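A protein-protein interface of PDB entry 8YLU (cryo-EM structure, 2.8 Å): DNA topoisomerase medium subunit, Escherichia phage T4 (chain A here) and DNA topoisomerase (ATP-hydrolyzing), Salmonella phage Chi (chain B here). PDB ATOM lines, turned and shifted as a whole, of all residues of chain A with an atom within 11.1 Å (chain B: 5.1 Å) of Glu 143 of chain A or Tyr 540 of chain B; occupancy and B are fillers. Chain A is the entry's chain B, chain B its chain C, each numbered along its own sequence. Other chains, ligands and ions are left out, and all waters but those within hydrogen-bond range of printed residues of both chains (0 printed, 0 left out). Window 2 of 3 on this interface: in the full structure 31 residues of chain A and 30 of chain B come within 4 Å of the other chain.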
ATOM      1  N   ASN A  14      13.454  -4.775 -17.563  1.00  0.00           N
ATOM      2  CA  ASN A  14      12.519  -5.579 -16.788  1.00  0.00           C
ATOM      3  C   ASN A  14      11.072  -5.354 -17.204  1.00  0.00           C
ATOM      4  O   ASN A  14      10.454  -6.254 -17.775  1.00  0.00           O
ATOM      5  CB  ASN A  14      12.693  -5.270 -15.295  1.00  0.00           C
ATOM      6  CG  ASN A  14      13.743  -6.137 -14.639  1.00  0.00           C
ATOM      7  OD1 ASN A  14      14.941  -5.916 -14.807  1.00  0.00           O
ATOM      8  ND2 ASN A  14      13.299  -7.131 -13.880  1.00  0.00           N
ATOM      9  N   PRO A  38      -4.785 -15.631 -27.199  1.00  0.00           N
ATOM     10  CA  PRO A  38      -5.300 -15.917 -25.850  1.00  0.00           C
ATOM     11  C   PRO A  38      -6.696 -15.376 -25.587  1.00  0.00           C
ATOM     12  O   PRO A  38      -7.487 -16.041 -24.907  1.00  0.00           O
ATOM     13  CB  PRO A  38      -4.246 -15.269 -24.948  1.00  0.00           C
ATOM     14  CG  PRO A  38      -2.996 -15.413 -25.734  1.00  0.00           C
ATOM     15  CD  PRO A  38      -3.394 -15.152 -27.157  1.00  0.00           C
ATOM     16  N   ARG A  41      -8.986 -17.770 -27.121  1.00  0.00           N
ATOM     17  CA  ARG A  41      -9.054 -18.974 -26.299  1.00  0.00           C
ATOM     18  C   ARG A  41      -9.971 -18.777 -25.100  1.00  0.00           C
ATOM     19  O   ARG A  41     -10.744 -19.673 -24.749  1.00  0.00           O
ATOM     20  CB  ARG A  41      -7.653 -19.372 -25.841  1.00  0.00           C
ATOM     21  CG  ARG A  41      -7.559 -20.779 -25.288  1.00  0.00           C
ATOM     22  CD  ARG A  41      -6.115 -21.180 -25.070  1.00  0.00           C
ATOM     23  NE  ARG A  41      -5.288 -20.884 -26.233  1.00  0.00           N
ATOM     24  CZ  ARG A  41      -4.253 -20.057 -26.224  1.00  0.00           C
ATOM     25  NH1 ARG A  41      -3.889 -19.418 -25.125  1.00  0.00           N
ATOM     26  NH2 ARG A  41      -3.563 -19.869 -27.344  1.00  0.00           N
ATOM     27  N   PHE A  42      -9.895 -17.611 -24.452  1.00  0.00           N
ATOM     28  CA  PHE A  42     -10.791 -17.330 -23.333  1.00  0.00           C
ATOM     29  C   PHE A  42     -12.242 -17.276 -23.791  1.00  0.00           C
ATOM     30  O   PHE A  42     -13.137 -17.787 -23.106  1.00  0.00           O
ATOM     31  CB  PHE A  42     -10.396 -16.017 -22.657  1.00  0.00           C
ATOM     32  CG  PHE A  42      -9.240 -16.150 -21.713  1.00  0.00           C
ATOM     33  CD1 PHE A  42      -9.351 -16.909 -20.566  1.00  0.00           C
ATOM     34  CD2 PHE A  42      -8.041 -15.515 -21.974  1.00  0.00           C
ATOM     35  CE1 PHE A  42      -8.287 -17.034 -19.700  1.00  0.00           C
ATOM     36  CE2 PHE A  42      -6.976 -15.638 -21.113  1.00  0.00           C
ATOM     37  CZ  PHE A  42      -7.100 -16.396 -19.976  1.00  0.00           C
ATOM     38  N   ALA A  45     -13.357 -20.845 -24.407  1.00  0.00           N
ATOM     39  CA  ALA A  45     -13.554 -21.564 -23.152  1.00  0.00           C
ATOM     40  C   ALA A  45     -14.845 -21.138 -22.469  1.00  0.00           C
ATOM     41  O   ALA A  45     -15.598 -21.980 -21.965  1.00  0.00           O
ATOM     42  CB  ALA A  45     -12.360 -21.339 -22.227  1.00  0.00           C
ATOM     43  N   ASP A  49     -18.139 -23.388 -21.699  1.00  0.00           N
ATOM     44  CA  ASP A  49     -18.751 -23.465 -20.376  1.00  0.00           C
ATOM     45  C   ASP A  49     -20.241 -23.165 -20.442  1.00  0.00           C
ATOM     46  O   ASP A  49     -21.046 -23.817 -19.770  1.00  0.00           O
ATOM     47  CB  ASP A  49     -18.054 -22.500 -19.417  1.00  0.00           C
ATOM     48  CG  ASP A  49     -16.642 -22.928 -19.083  1.00  0.00           C
ATOM     49  OD1 ASP A  49     -16.084 -23.773 -19.815  1.00  0.00           O
ATOM     50  OD2 ASP A  49     -16.086 -22.416 -18.088  1.00  0.00           O
ATOM     51  N   GLY A  67     -17.971 -13.316 -18.382  1.00  0.00           N
ATOM     52  CA  GLY A  67     -17.363 -14.337 -17.560  1.00  0.00           C
ATOM     53  C   GLY A  67     -15.941 -14.718 -17.893  1.00  0.00           C
ATOM     54  O   GLY A  67     -15.388 -15.600 -17.230  1.00  0.00           O
ATOM     55  N   VAL A  68     -15.318 -14.095 -18.897  1.00  0.00           N
ATOM     56  CA  VAL A  68     -13.950 -14.460 -19.241  1.00  0.00           C
ATOM     57  C   VAL A  68     -12.960 -14.001 -18.181  1.00  0.00           C
ATOM     58  O   VAL A  68     -11.877 -14.584 -18.061  1.00  0.00           O
ATOM     59  CB  VAL A  68     -13.556 -13.902 -20.623  1.00  0.00           C
ATOM     60  CG1 VAL A  68     -14.502 -14.415 -21.692  1.00  0.00           C
ATOM     61  CG2 VAL A  68     -13.531 -12.389 -20.603  1.00  0.00           C
ATOM     62  N   ALA A  69     -13.299 -12.970 -17.403  1.00  0.00           N
ATOM     63  CA  ALA A  69     -12.405 -12.524 -16.341  1.00  0.00           C
ATOM     64  C   ALA A  69     -12.276 -13.569 -15.242  1.00  0.00           C
ATOM     65  O   ALA A  69     -11.223 -13.670 -14.603  1.00  0.00           O
ATOM     66  CB  ALA A  69     -12.895 -11.200 -15.761  1.00  0.00           C
ATOM     67  N   ASP A  70     -13.333 -14.348 -15.005  1.00  0.00           N
ATOM     68  CA  ASP A  70     -13.256 -15.431 -14.031  1.00  0.00           C
ATOM     69  C   ASP A  70     -12.350 -16.555 -14.514  1.00  0.00           C
ATOM     70  O   ASP A  70     -11.780 -17.283 -13.694  1.00  0.00           O
ATOM     71  CB  ASP A  70     -14.656 -15.965 -13.738  1.00  0.00           C
ATOM     72  CG  ASP A  70     -14.749 -16.642 -12.387  1.00  0.00           C
ATOM     73  OD1 ASP A  70     -13.939 -16.307 -11.498  1.00  0.00           O
ATOM     74  OD2 ASP A  70     -15.631 -17.506 -12.214  1.00  0.00           O
ATOM     75  N   LEU A  71     -12.208 -16.716 -15.829  1.00  0.00           N
ATOM     76  CA  LEU A  71     -11.344 -17.746 -16.389  1.00  0.00           C
ATOM     77  C   LEU A  71      -9.877 -17.348 -16.403  1.00  0.00           C
ATOM     78  O   LEU A  71      -9.030 -18.186 -16.728  1.00  0.00           O
ATOM     79  CB  LEU A  71     -11.783 -18.091 -17.813  1.00  0.00           C
ATOM     80  CG  LEU A  71     -13.252 -18.435 -18.043  1.00  0.00           C
ATOM     81  CD1 LEU A  71     -13.542 -18.483 -19.526  1.00  0.00           C
ATOM     82  CD2 LEU A  71     -13.605 -19.755 -17.391  1.00  0.00           C
ATOM     83  N   GLY A  72      -9.553 -16.102 -16.073  1.00  0.00           N
ATOM     84  CA  GLY A  72      -8.170 -15.673 -16.033  1.00  0.00           C
ATOM     85  C   GLY A  72      -7.835 -14.587 -17.031  1.00  0.00           C
ATOM     86  O   GLY A  72      -6.662 -14.374 -17.349  1.00  0.00           O
ATOM     87  N   TYR A  73      -8.853 -13.897 -17.537  1.00  0.00           N
ATOM     88  CA  TYR A  73      -8.637 -12.786 -18.453  1.00  0.00           C
ATOM     89  C   TYR A  73      -8.381 -11.511 -17.660  1.00  0.00           C
ATOM     90  O   TYR A  73      -9.155 -11.159 -16.765  1.00  0.00           O
ATOM     91  CB  TYR A  73      -9.841 -12.608 -19.374  1.00  0.00           C
ATOM     92  CG  TYR A  73      -9.589 -11.696 -20.550  1.00  0.00           C
ATOM     93  CD1 TYR A  73      -8.476 -11.866 -21.361  1.00  0.00           C
ATOM     94  CD2 TYR A  73     -10.464 -10.662 -20.848  1.00  0.00           C
ATOM     95  CE1 TYR A  73      -8.243 -11.033 -22.434  1.00  0.00           C
ATOM     96  CE2 TYR A  73     -10.238  -9.827 -21.919  1.00  0.00           C
ATOM     97  CZ  TYR A  73      -9.127 -10.015 -22.707  1.00  0.00           C
ATOM     98  OH  TYR A  73      -8.905  -9.180 -23.774  1.00  0.00           O
ATOM     99  N   HIS A  74      -7.295 -10.817 -17.993  1.00  0.00           N
ATOM    100  CA  HIS A  74      -6.816  -9.694 -17.200  1.00  0.00           C
ATOM    101  C   HIS A  74      -6.994  -8.356 -17.904  1.00  0.00           C
ATOM    102  O   HIS A  74      -6.287  -7.395 -17.585  1.00  0.00           O
ATOM    103  CB  HIS A  74      -5.348  -9.909 -16.836  1.00  0.00           C
ATOM    104  CG  HIS A  74      -5.124 -11.044 -15.887  1.00  0.00           C
ATOM    105  ND1 HIS A  74      -3.920 -11.707 -15.793  1.00  0.00           N
ATOM    106  CD2 HIS A  74      -5.950 -11.633 -14.991  1.00  0.00           C
ATOM    107  CE1 HIS A  74      -4.015 -12.655 -14.878  1.00  0.00           C
ATOM    108  NE2 HIS A  74      -5.236 -12.632 -14.377  1.00  0.00           N
ATOM    109  N   VAL A 138      -2.012 -28.284 -19.417  1.00  0.00           N
ATOM    110  CA  VAL A 138      -2.448 -27.429 -18.321  1.00  0.00           C
ATOM    111  C   VAL A 138      -1.527 -26.220 -18.247  1.00  0.00           C
ATOM    112  O   VAL A 138      -0.299 -26.364 -18.204  1.00  0.00           O
ATOM    113  CB  VAL A 138      -2.457 -28.203 -16.993  1.00  0.00           C
ATOM    114  CG1 VAL A 138      -2.428 -27.246 -15.814  1.00  0.00           C
ATOM    115  CG2 VAL A 138      -3.675 -29.108 -16.917  1.00  0.00           C
ATOM    116  N   HIS A 139      -2.119 -25.028 -18.244  1.00  0.00           N
ATOM    117  CA  HIS A 139      -1.343 -23.802 -18.149  1.00  0.00           C
ATOM    118  C   HIS A 139      -0.632 -23.725 -16.804  1.00  0.00           C
ATOM    119  O   HIS A 139      -1.137 -24.190 -15.780  1.00  0.00           O
ATOM    120  CB  HIS A 139      -2.252 -22.586 -18.335  1.00  0.00           C
ATOM    121  CG  HIS A 139      -1.531 -21.351 -18.776  1.00  0.00           C
ATOM    122  ND1 HIS A 139      -1.180 -20.342 -17.905  1.00  0.00           N
ATOM    123  CD2 HIS A 139      -1.098 -20.959 -19.998  1.00  0.00           C
ATOM    124  CE1 HIS A 139      -0.561 -19.385 -18.570  1.00  0.00           C
ATOM    125  NE2 HIS A 139      -0.498 -19.734 -19.842  1.00  0.00           N
ATOM    126  N   GLN A 140       0.559 -23.123 -16.811  1.00  0.00           N
ATOM    127  CA  GLN A 140       1.360 -23.029 -15.598  1.00  0.00           C
ATOM    128  C   GLN A 140       0.754 -22.100 -14.555  1.00  0.00           C
ATOM    129  O   GLN A 140       1.220 -22.098 -13.411  1.00  0.00           O
ATOM    130  CB  GLN A 140       2.780 -22.572 -15.938  1.00  0.00           C
ATOM    131  CG  GLN A 140       2.896 -21.097 -16.274  1.00  0.00           C
ATOM    132  CD  GLN A 140       3.976 -20.820 -17.301  1.00  0.00           C
ATOM    133  OE1 GLN A 140       5.084 -21.346 -17.208  1.00  0.00           O
ATOM    134  NE2 GLN A 140       3.656 -19.993 -18.289  1.00  0.00           N
ATOM    135  N   ASP A 141      -0.257 -21.316 -14.915  1.00  0.00           N
ATOM    136  CA  ASP A 141      -0.957 -20.450 -13.977  1.00  0.00           C
ATOM    137  C   ASP A 141      -2.223 -21.144 -13.497  1.00  0.00           C
ATOM    138  O   ASP A 141      -3.034 -21.594 -14.311  1.00  0.00           O
ATOM    139  CB  ASP A 141      -1.305 -19.110 -14.625  1.00  0.00           C
ATOM    140  CG  ASP A 141      -0.261 -18.046 -14.361  1.00  0.00           C
ATOM    141  OD1 ASP A 141      -0.252 -17.487 -13.245  1.00  0.00           O
ATOM    142  OD2 ASP A 141       0.547 -17.766 -15.270  1.00  0.00           O
ATOM    143  N   LYS A 142      -2.386 -21.233 -12.175  1.00  0.00           N
ATOM    144  CA  LYS A 142      -3.572 -21.875 -11.620  1.00  0.00           C
ATOM    145  C   LYS A 142      -4.840 -21.095 -11.945  1.00  0.00           C
ATOM    146  O   LYS A 142      -5.929 -21.677 -11.996  1.00  0.00           O
ATOM    147  CB  LYS A 142      -3.418 -22.039 -10.108  1.00  0.00           C
ATOM    148  CG  LYS A 142      -4.474 -22.921  -9.463  1.00  0.00           C
ATOM    149  CD  LYS A 142      -4.570 -22.665  -7.968  1.00  0.00           C
ATOM    150  CE  LYS A 142      -5.926 -23.080  -7.422  1.00  0.00           C
ATOM    151  NZ  LYS A 142      -6.150 -24.547  -7.542  1.00  0.00           N
ATOM    152  N   GLU A 143      -4.721 -19.788 -12.170  1.00  0.00           N
ATOM    153  CA  GLU A 143      -5.873 -18.956 -12.488  1.00  0.00           C
ATOM    154  C   GLU A 143      -6.250 -19.002 -13.962  1.00  0.00           C
ATOM    155  O   GLU A 143      -7.282 -18.437 -14.337  1.00  0.00           O
ATOM    156  CB  GLU A 143      -5.603 -17.510 -12.070  1.00  0.00           C
ATOM    157  CG  GLU A 143      -5.513 -17.307 -10.567  1.00  0.00           C
ATOM    158  CD  GLU A 143      -4.152 -17.672 -10.011  1.00  0.00           C
ATOM    159  OE1 GLU A 143      -3.171 -17.641 -10.782  1.00  0.00           O
ATOM    160  OE2 GLU A 143      -4.063 -17.990  -8.807  1.00  0.00           O
ATOM    161  N   HIS A 144      -5.446 -19.653 -14.799  1.00  0.00           N
ATOM    162  CA  HIS A 144      -5.734 -19.799 -16.225  1.00  0.00           C
ATOM    163  C   HIS A 144      -6.575 -21.056 -16.401  1.00  0.00           C
ATOM    164  O   HIS A 144      -6.059 -22.150 -16.631  1.00  0.00           O
ATOM    165  CB  HIS A 144      -4.440 -19.863 -17.026  1.00  0.00           C
ATOM    166  CG  HIS A 144      -4.617 -19.617 -18.490  1.00  0.00           C
ATOM    167  ND1 HIS A 144      -5.168 -20.549 -19.343  1.00  0.00           N
ATOM    168  CD2 HIS A 144      -4.302 -18.547 -19.258  1.00  0.00           C
ATOM    169  CE1 HIS A 144      -5.190 -20.062 -20.570  1.00  0.00           C
ATOM    170  NE2 HIS A 144      -4.669 -18.848 -20.546  1.00  0.00           N
ATOM    171  N   ILE A 145      -7.894 -20.897 -16.277  1.00  0.00           N
ATOM    172  CA  ILE A 145      -8.792 -22.052 -16.346  1.00  0.00           C
ATOM    173  C   ILE A 145      -8.731 -22.759 -17.696  1.00  0.00           C
ATOM    174  O   ILE A 145      -8.641 -23.998 -17.713  1.00  0.00           O
ATOM    175  CB  ILE A 145     -10.221 -21.637 -15.949  1.00  0.00           C
ATOM    176  CG1 ILE A 145     -10.424 -21.799 -14.442  1.00  0.00           C
ATOM    177  CG2 ILE A 145     -11.251 -22.469 -16.691  1.00  0.00           C
ATOM    178  CD1 ILE A 145      -9.698 -20.776 -13.604  1.00  0.00           C
ATOM    179  N   PRO A 146      -8.776 -22.072 -18.839  1.00  0.00           N
ATOM    180  CA  PRO A 146      -8.642 -22.777 -20.120  1.00  0.00           C
ATOM    181  C   PRO A 146      -7.255 -23.371 -20.269  1.00  0.00           C
ATOM    182  O   PRO A 146      -6.298 -22.900 -19.635  1.00  0.00           O
ATOM    183  CB  PRO A 146      -8.896 -21.676 -21.162  1.00  0.00           C
ATOM    184  CG  PRO A 146      -8.628 -20.417 -20.457  1.00  0.00           C
ATOM    185  CD  PRO A 146      -9.073 -20.643 -19.053  1.00  0.00           C
ATOM    186  N   PRO A 147      -7.103 -24.412 -21.089  1.00  0.00           N
ATOM    187  CA  PRO A 147      -5.797 -25.073 -21.208  1.00  0.00           C
ATOM    188  C   PRO A 147      -4.734 -24.192 -21.843  1.00  0.00           C
ATOM    189  O   PRO A 147      -5.020 -23.070 -22.271  1.00  0.00           O
ATOM    190  CB  PRO A 147      -6.107 -26.290 -22.086  1.00  0.00           C
ATOM    191  CG  PRO A 147      -7.315 -25.908 -22.847  1.00  0.00           C
ATOM    192  CD  PRO A 147      -8.127 -25.063 -21.920  1.00  0.00           C
ATOM    193  N   ALA A 148      -3.497 -24.692 -21.898  1.00  0.00           N
ATOM    194  CA  ALA A 148      -2.440 -23.956 -22.583  1.00  0.00           C
ATOM    195  C   ALA A 148      -2.784 -23.761 -24.052  1.00  0.00           C
ATOM    196  O   ALA A 148      -2.582 -22.677 -24.608  1.00  0.00           O
ATOM    197  CB  ALA A 148      -1.108 -24.689 -22.433  1.00  0.00           C
ATOM    198  N   ILE B 523      -0.649  -7.754  -7.514  1.00  0.00           N
ATOM    199  CA  ILE B 523      -1.235  -8.943  -6.908  1.00  0.00           C
ATOM    200  C   ILE B 523      -1.383  -8.690  -5.417  1.00  0.00           C
ATOM    201  O   ILE B 523      -0.462  -8.172  -4.777  1.00  0.00           O
ATOM    202  CB  ILE B 523      -0.381 -10.199  -7.166  1.00  0.00           C
ATOM    203  CG1 ILE B 523      -0.208 -10.434  -8.669  1.00  0.00           C
ATOM    204  CG2 ILE B 523      -1.002 -11.418  -6.501  1.00  0.00           C
ATOM    205  CD1 ILE B 523      -1.327 -11.229  -9.302  1.00  0.00           C
ATOM    206  N   PHE B 534       2.309  -7.874  -4.030  1.00  0.00           N
ATOM    207  CA  PHE B 534       3.309  -8.103  -5.062  1.00  0.00           C
ATOM    208  C   PHE B 534       3.141  -7.029  -6.124  1.00  0.00           C
ATOM    209  O   PHE B 534       2.071  -6.914  -6.733  1.00  0.00           O
ATOM    210  CB  PHE B 534       3.167  -9.501  -5.668  1.00  0.00           C
ATOM    211  CG  PHE B 534       3.214 -10.604  -4.654  1.00  0.00           C
ATOM    212  CD1 PHE B 534       4.426 -11.094  -4.202  1.00  0.00           C
ATOM    213  CD2 PHE B 534       2.048 -11.147  -4.148  1.00  0.00           C
ATOM    214  CE1 PHE B 534       4.474 -12.104  -3.270  1.00  0.00           C
ATOM    215  CE2 PHE B 534       2.091 -12.157  -3.214  1.00  0.00           C
ATOM    216  CZ  PHE B 534       3.306 -12.637  -2.774  1.00  0.00           C
ATOM    217  N   THR B 536       4.904  -6.538  -9.036  1.00  0.00           N
ATOM    218  CA  THR B 536       4.985  -7.024 -10.404  1.00  0.00           C
ATOM    219  C   THR B 536       4.558  -8.483 -10.456  1.00  0.00           C
ATOM    220  O   THR B 536       4.688  -9.220  -9.476  1.00  0.00           O
ATOM    221  CB  THR B 536       6.401  -6.874 -10.972  1.00  0.00           C
ATOM    222  OG1 THR B 536       7.339  -7.509 -10.098  1.00  0.00           O
ATOM    223  CG2 THR B 536       6.764  -5.407 -11.113  1.00  0.00           C
ATOM    224  N   VAL B 537       4.036  -8.890 -11.615  1.00  0.00           N
ATOM    225  CA  VAL B 537       3.588 -10.270 -11.785  1.00  0.00           C
ATOM    226  C   VAL B 537       4.769 -11.226 -11.695  1.00  0.00           C
ATOM    227  O   VAL B 537       4.644 -12.344 -11.181  1.00  0.00           O
ATOM    228  CB  VAL B 537       2.828 -10.423 -13.116  1.00  0.00           C
ATOM    229  CG1 VAL B 537       2.437 -11.872 -13.345  1.00  0.00           C
ATOM    230  CG2 VAL B 537       1.597  -9.537 -13.127  1.00  0.00           C
ATOM    231  N   ALA B 538       5.934 -10.801 -12.188  1.00  0.00           N
ATOM    232  CA  ALA B 538       7.118 -11.652 -12.126  1.00  0.00           C
ATOM    233  C   ALA B 538       7.494 -11.972 -10.687  1.00  0.00           C
ATOM    234  O   ALA B 538       7.854 -13.112 -10.372  1.00  0.00           O
ATOM    235  CB  ALA B 538       8.284 -10.979 -12.848  1.00  0.00           C
ATOM    236  N   GLU B 539       7.417 -10.979  -9.798  1.00  0.00           N
ATOM    237  CA  GLU B 539       7.721 -11.218  -8.390  1.00  0.00           C
ATOM    238  C   GLU B 539       6.756 -12.226  -7.782  1.00  0.00           C
ATOM    239  O   GLU B 539       7.171 -13.120  -7.032  1.00  0.00           O
ATOM    240  CB  GLU B 539       7.675  -9.902  -7.613  1.00  0.00           C
ATOM    241  CG  GLU B 539       8.916  -9.044  -7.765  1.00  0.00           C
ATOM    242  CD  GLU B 539       8.738  -7.658  -7.180  1.00  0.00           C
ATOM    243  OE1 GLU B 539       7.873  -7.490  -6.295  1.00  0.00           O
ATOM    244  OE2 GLU B 539       9.464  -6.734  -7.603  1.00  0.00           O
ATOM    245  N   TYR B 540       5.465 -12.102  -8.094  1.00  0.00           N
ATOM    246  CA  TYR B 540       4.489 -13.046  -7.562  1.00  0.00           C
ATOM    247  C   TYR B 540       4.747 -14.455  -8.074  1.00  0.00           C
ATOM    248  O   TYR B 540       4.718 -15.416  -7.299  1.00  0.00           O
ATOM    249  CB  TYR B 540       3.071 -12.607  -7.918  1.00  0.00           C
ATOM    250  CG  TYR B 540       2.048 -13.698  -7.718  1.00  0.00           C
ATOM    251  CD1 TYR B 540       1.768 -14.190  -6.451  1.00  0.00           C
ATOM    252  CD2 TYR B 540       1.367 -14.243  -8.796  1.00  0.00           C
ATOM    253  CE1 TYR B 540       0.838 -15.190  -6.263  1.00  0.00           C
ATOM    254  CE2 TYR B 540       0.433 -15.244  -8.618  1.00  0.00           C
ATOM    255  CZ  TYR B 540       0.173 -15.712  -7.349  1.00  0.00           C
ATOM    256  OH  TYR B 540      -0.755 -16.709  -7.171  1.00  0.00           O
ATOM    257  N   GLU B 541       5.009 -14.599  -9.375  1.00  0.00           N
ATOM    258  CA  GLU B 541       5.274 -15.922  -9.931  1.00  0.00           C
ATOM    259  C   GLU B 541       6.532 -16.530  -9.325  1.00  0.00           C
ATOM    260  O   GLU B 541       6.579 -17.735  -9.055  1.00  0.00           O
ATOM    261  CB  GLU B 541       5.396 -15.846 -11.452  1.00  0.00           C
ATOM    262  CG  GLU B 541       4.160 -15.310 -12.150  1.00  0.00           C
ATOM    263  CD  GLU B 541       3.015 -16.298 -12.144  1.00  0.00           C
ATOM    264  OE1 GLU B 541       3.280 -17.519 -12.140  1.00  0.00           O
ATOM    265  OE2 GLU B 541       1.848 -15.855 -12.142  1.00  0.00           O
ATOM    266  N   SER B 542       7.564 -15.713  -9.111  1.00  0.00           N
ATOM    267  CA  SER B 542       8.783 -16.212  -8.485  1.00  0.00           C
ATOM    268  C   SER B 542       8.527 -16.655  -7.051  1.00  0.00           C
ATOM    269  O   SER B 542       9.084 -17.662  -6.599  1.00  0.00           O
ATOM    270  CB  SER B 542       9.872 -15.143  -8.532  1.00  0.00           C
ATOM    271  OG  SER B 542       9.980 -14.473  -7.289  1.00  0.00           O
ATOM    272  N   ALA B 543       7.698 -15.916  -6.317  1.00  0.00           N
ATOM    273  CA  ALA B 543       7.426 -16.221  -4.920  1.00  0.00           C
ATOM    274  C   ALA B 543       6.144 -17.015  -4.706  1.00  0.00           C
ATOM    275  O   ALA B 543       5.796 -17.289  -3.557  1.00  0.00           O
ATOM    276  CB  ALA B 543       7.367 -14.928  -4.100  1.00  0.00           C
ATOM    277  N   LYS B 544       5.441 -17.401  -5.772  1.00  0.00           N
ATOM    278  CA  LYS B 544       4.161 -18.085  -5.603  1.00  0.00           C
ATOM    279  C   LYS B 544       4.335 -19.458  -4.966  1.00  0.00           C
ATOM    280  O   LYS B 544       3.490 -19.894  -4.175  1.00  0.00           O
ATOM    281  CB  LYS B 544       3.449 -18.214  -6.950  1.00  0.00           C
ATOM    282  CG  LYS B 544       2.106 -18.921  -6.877  1.00  0.00           C
ATOM    283  CD  LYS B 544       1.410 -18.941  -8.226  1.00  0.00           C
ATOM    284  CE  LYS B 544       2.366 -19.313  -9.345  1.00  0.00           C
ATOM    285  NZ  LYS B 544       1.667 -19.381 -10.657  1.00  0.00           N
ATOM    286  N   HIS B 550      -3.771 -19.982  -0.300  1.00  0.00           N
ATOM    287  CA  HIS B 550      -4.179 -18.585  -0.349  1.00  0.00           C
ATOM    288  C   HIS B 550      -5.016 -18.356  -1.597  1.00  0.00           C
ATOM    289  O   HIS B 550      -5.146 -19.232  -2.456  1.00  0.00           O
ATOM    290  CB  HIS B 550      -2.967 -17.650  -0.335  1.00  0.00           C
ATOM    291  CG  HIS B 550      -2.085 -17.785  -1.538  1.00  0.00           C
ATOM    292  ND1 HIS B 550      -0.917 -18.515  -1.525  1.00  0.00           N
ATOM    293  CD2 HIS B 550      -2.201 -17.283  -2.790  1.00  0.00           C
ATOM    294  CE1 HIS B 550      -0.351 -18.458  -2.718  1.00  0.00           C
ATOM    295  NE2 HIS B 550      -1.111 -17.716  -3.503  1.00  0.00           N
ATOM    296  N   ILE B 552      -5.586 -15.092  -4.532  1.00  0.00           N
ATOM    297  CA  ILE B 552      -4.985 -13.857  -5.015  1.00  0.00           C
ATOM    298  C   ILE B 552      -6.058 -12.961  -5.611  1.00  0.00           C
ATOM    299  O   ILE B 552      -7.101 -13.423  -6.090  1.00  0.00           O
ATOM    300  CB  ILE B 552      -3.870 -14.123  -6.047  1.00  0.00           C
ATOM    301  CG1 ILE B 552      -4.447 -14.773  -7.304  1.00  0.00           C
ATOM    302  CG2 ILE B 552      -2.784 -14.983  -5.437  1.00  0.00           C
ATOM    303  CD1 ILE B 552      -3.666 -14.470  -8.559  1.00  0.00           C
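NZ of Lys 544 of chain B is in salt-bridge range of OD1 of Asp 141 of chain A, 3.7 Å away. OD1 of Asp 141 of chain A sits close to OE2 of Glu 541 of chain B, at 2.9 Å.
OE1 of Glu 541 of chain B lies within salt-bridge range of NZ of Lys 544 of chain B (2.9 Å). ND1 of His 139 of chain A lies close to N of Asp 141 of chain A, 3.3 Å away.
Among the printed residues, merely in contact across the chains: Glu 143 of chain A with Ile 552 of chain B (3.5 Å), Gln 140 of chain A with Lys 544 of chain B (3.9 Å) and Glu 143 of chain A with Tyr 540 of chain B (3.9 Å).
Of the printed residues of chain B, Gln 140 of chain A touches Lys 544 (3.9 Å). Of the printed residues of chain B, Asp 141 of chain A touches Glu 541 and Lys 544. Glu 143 of chain A touches just these residues of chain B: Tyr 540 (3.9 Å) and Ile 552 (3.5 Å). Ala 148 of chain A touches none of the printed residues of chain B. No residue of chain A comes within 4 Å of Phe 534 of chain B. No residue of chain A comes within 4 Å of Val 537 of chain B. Ala 538 of chain B touches none of the printed residues of chain A. Tyr 540 of chain B touches one residue of chain A. Of chain A, only Asp 141 (2.9 Å) comes within 4 Å of Glu 541 of chain B. No residue of chain A comes within 4 Å of Ser 542 of chain B. Of chain A, only Glu 143 (3.5 Å) comes within 4 Å of Ile 552 of chain B. The nearest residue of chain A that does not touch Tyr 540 of chain B is Asp 141 of chain A (5.2 Å). The nearest printed residue of chain B that does not touch Asp 141 of chain A is Tyr 540 of chain B (5.2 Å).
Printed residues of chain A that touch a printed residue of chain B: Gln 140, Asp 141 and Glu 143. Among the printed residues, 5 pairs touch across the chains. Among the printed residues, Asp or Glu carboxylates within 4 Å of a Lys or Arg side-chain nitrogen of the other chain: Asp 141 of chain A with Lys 544 of chain B (3.7 Å).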
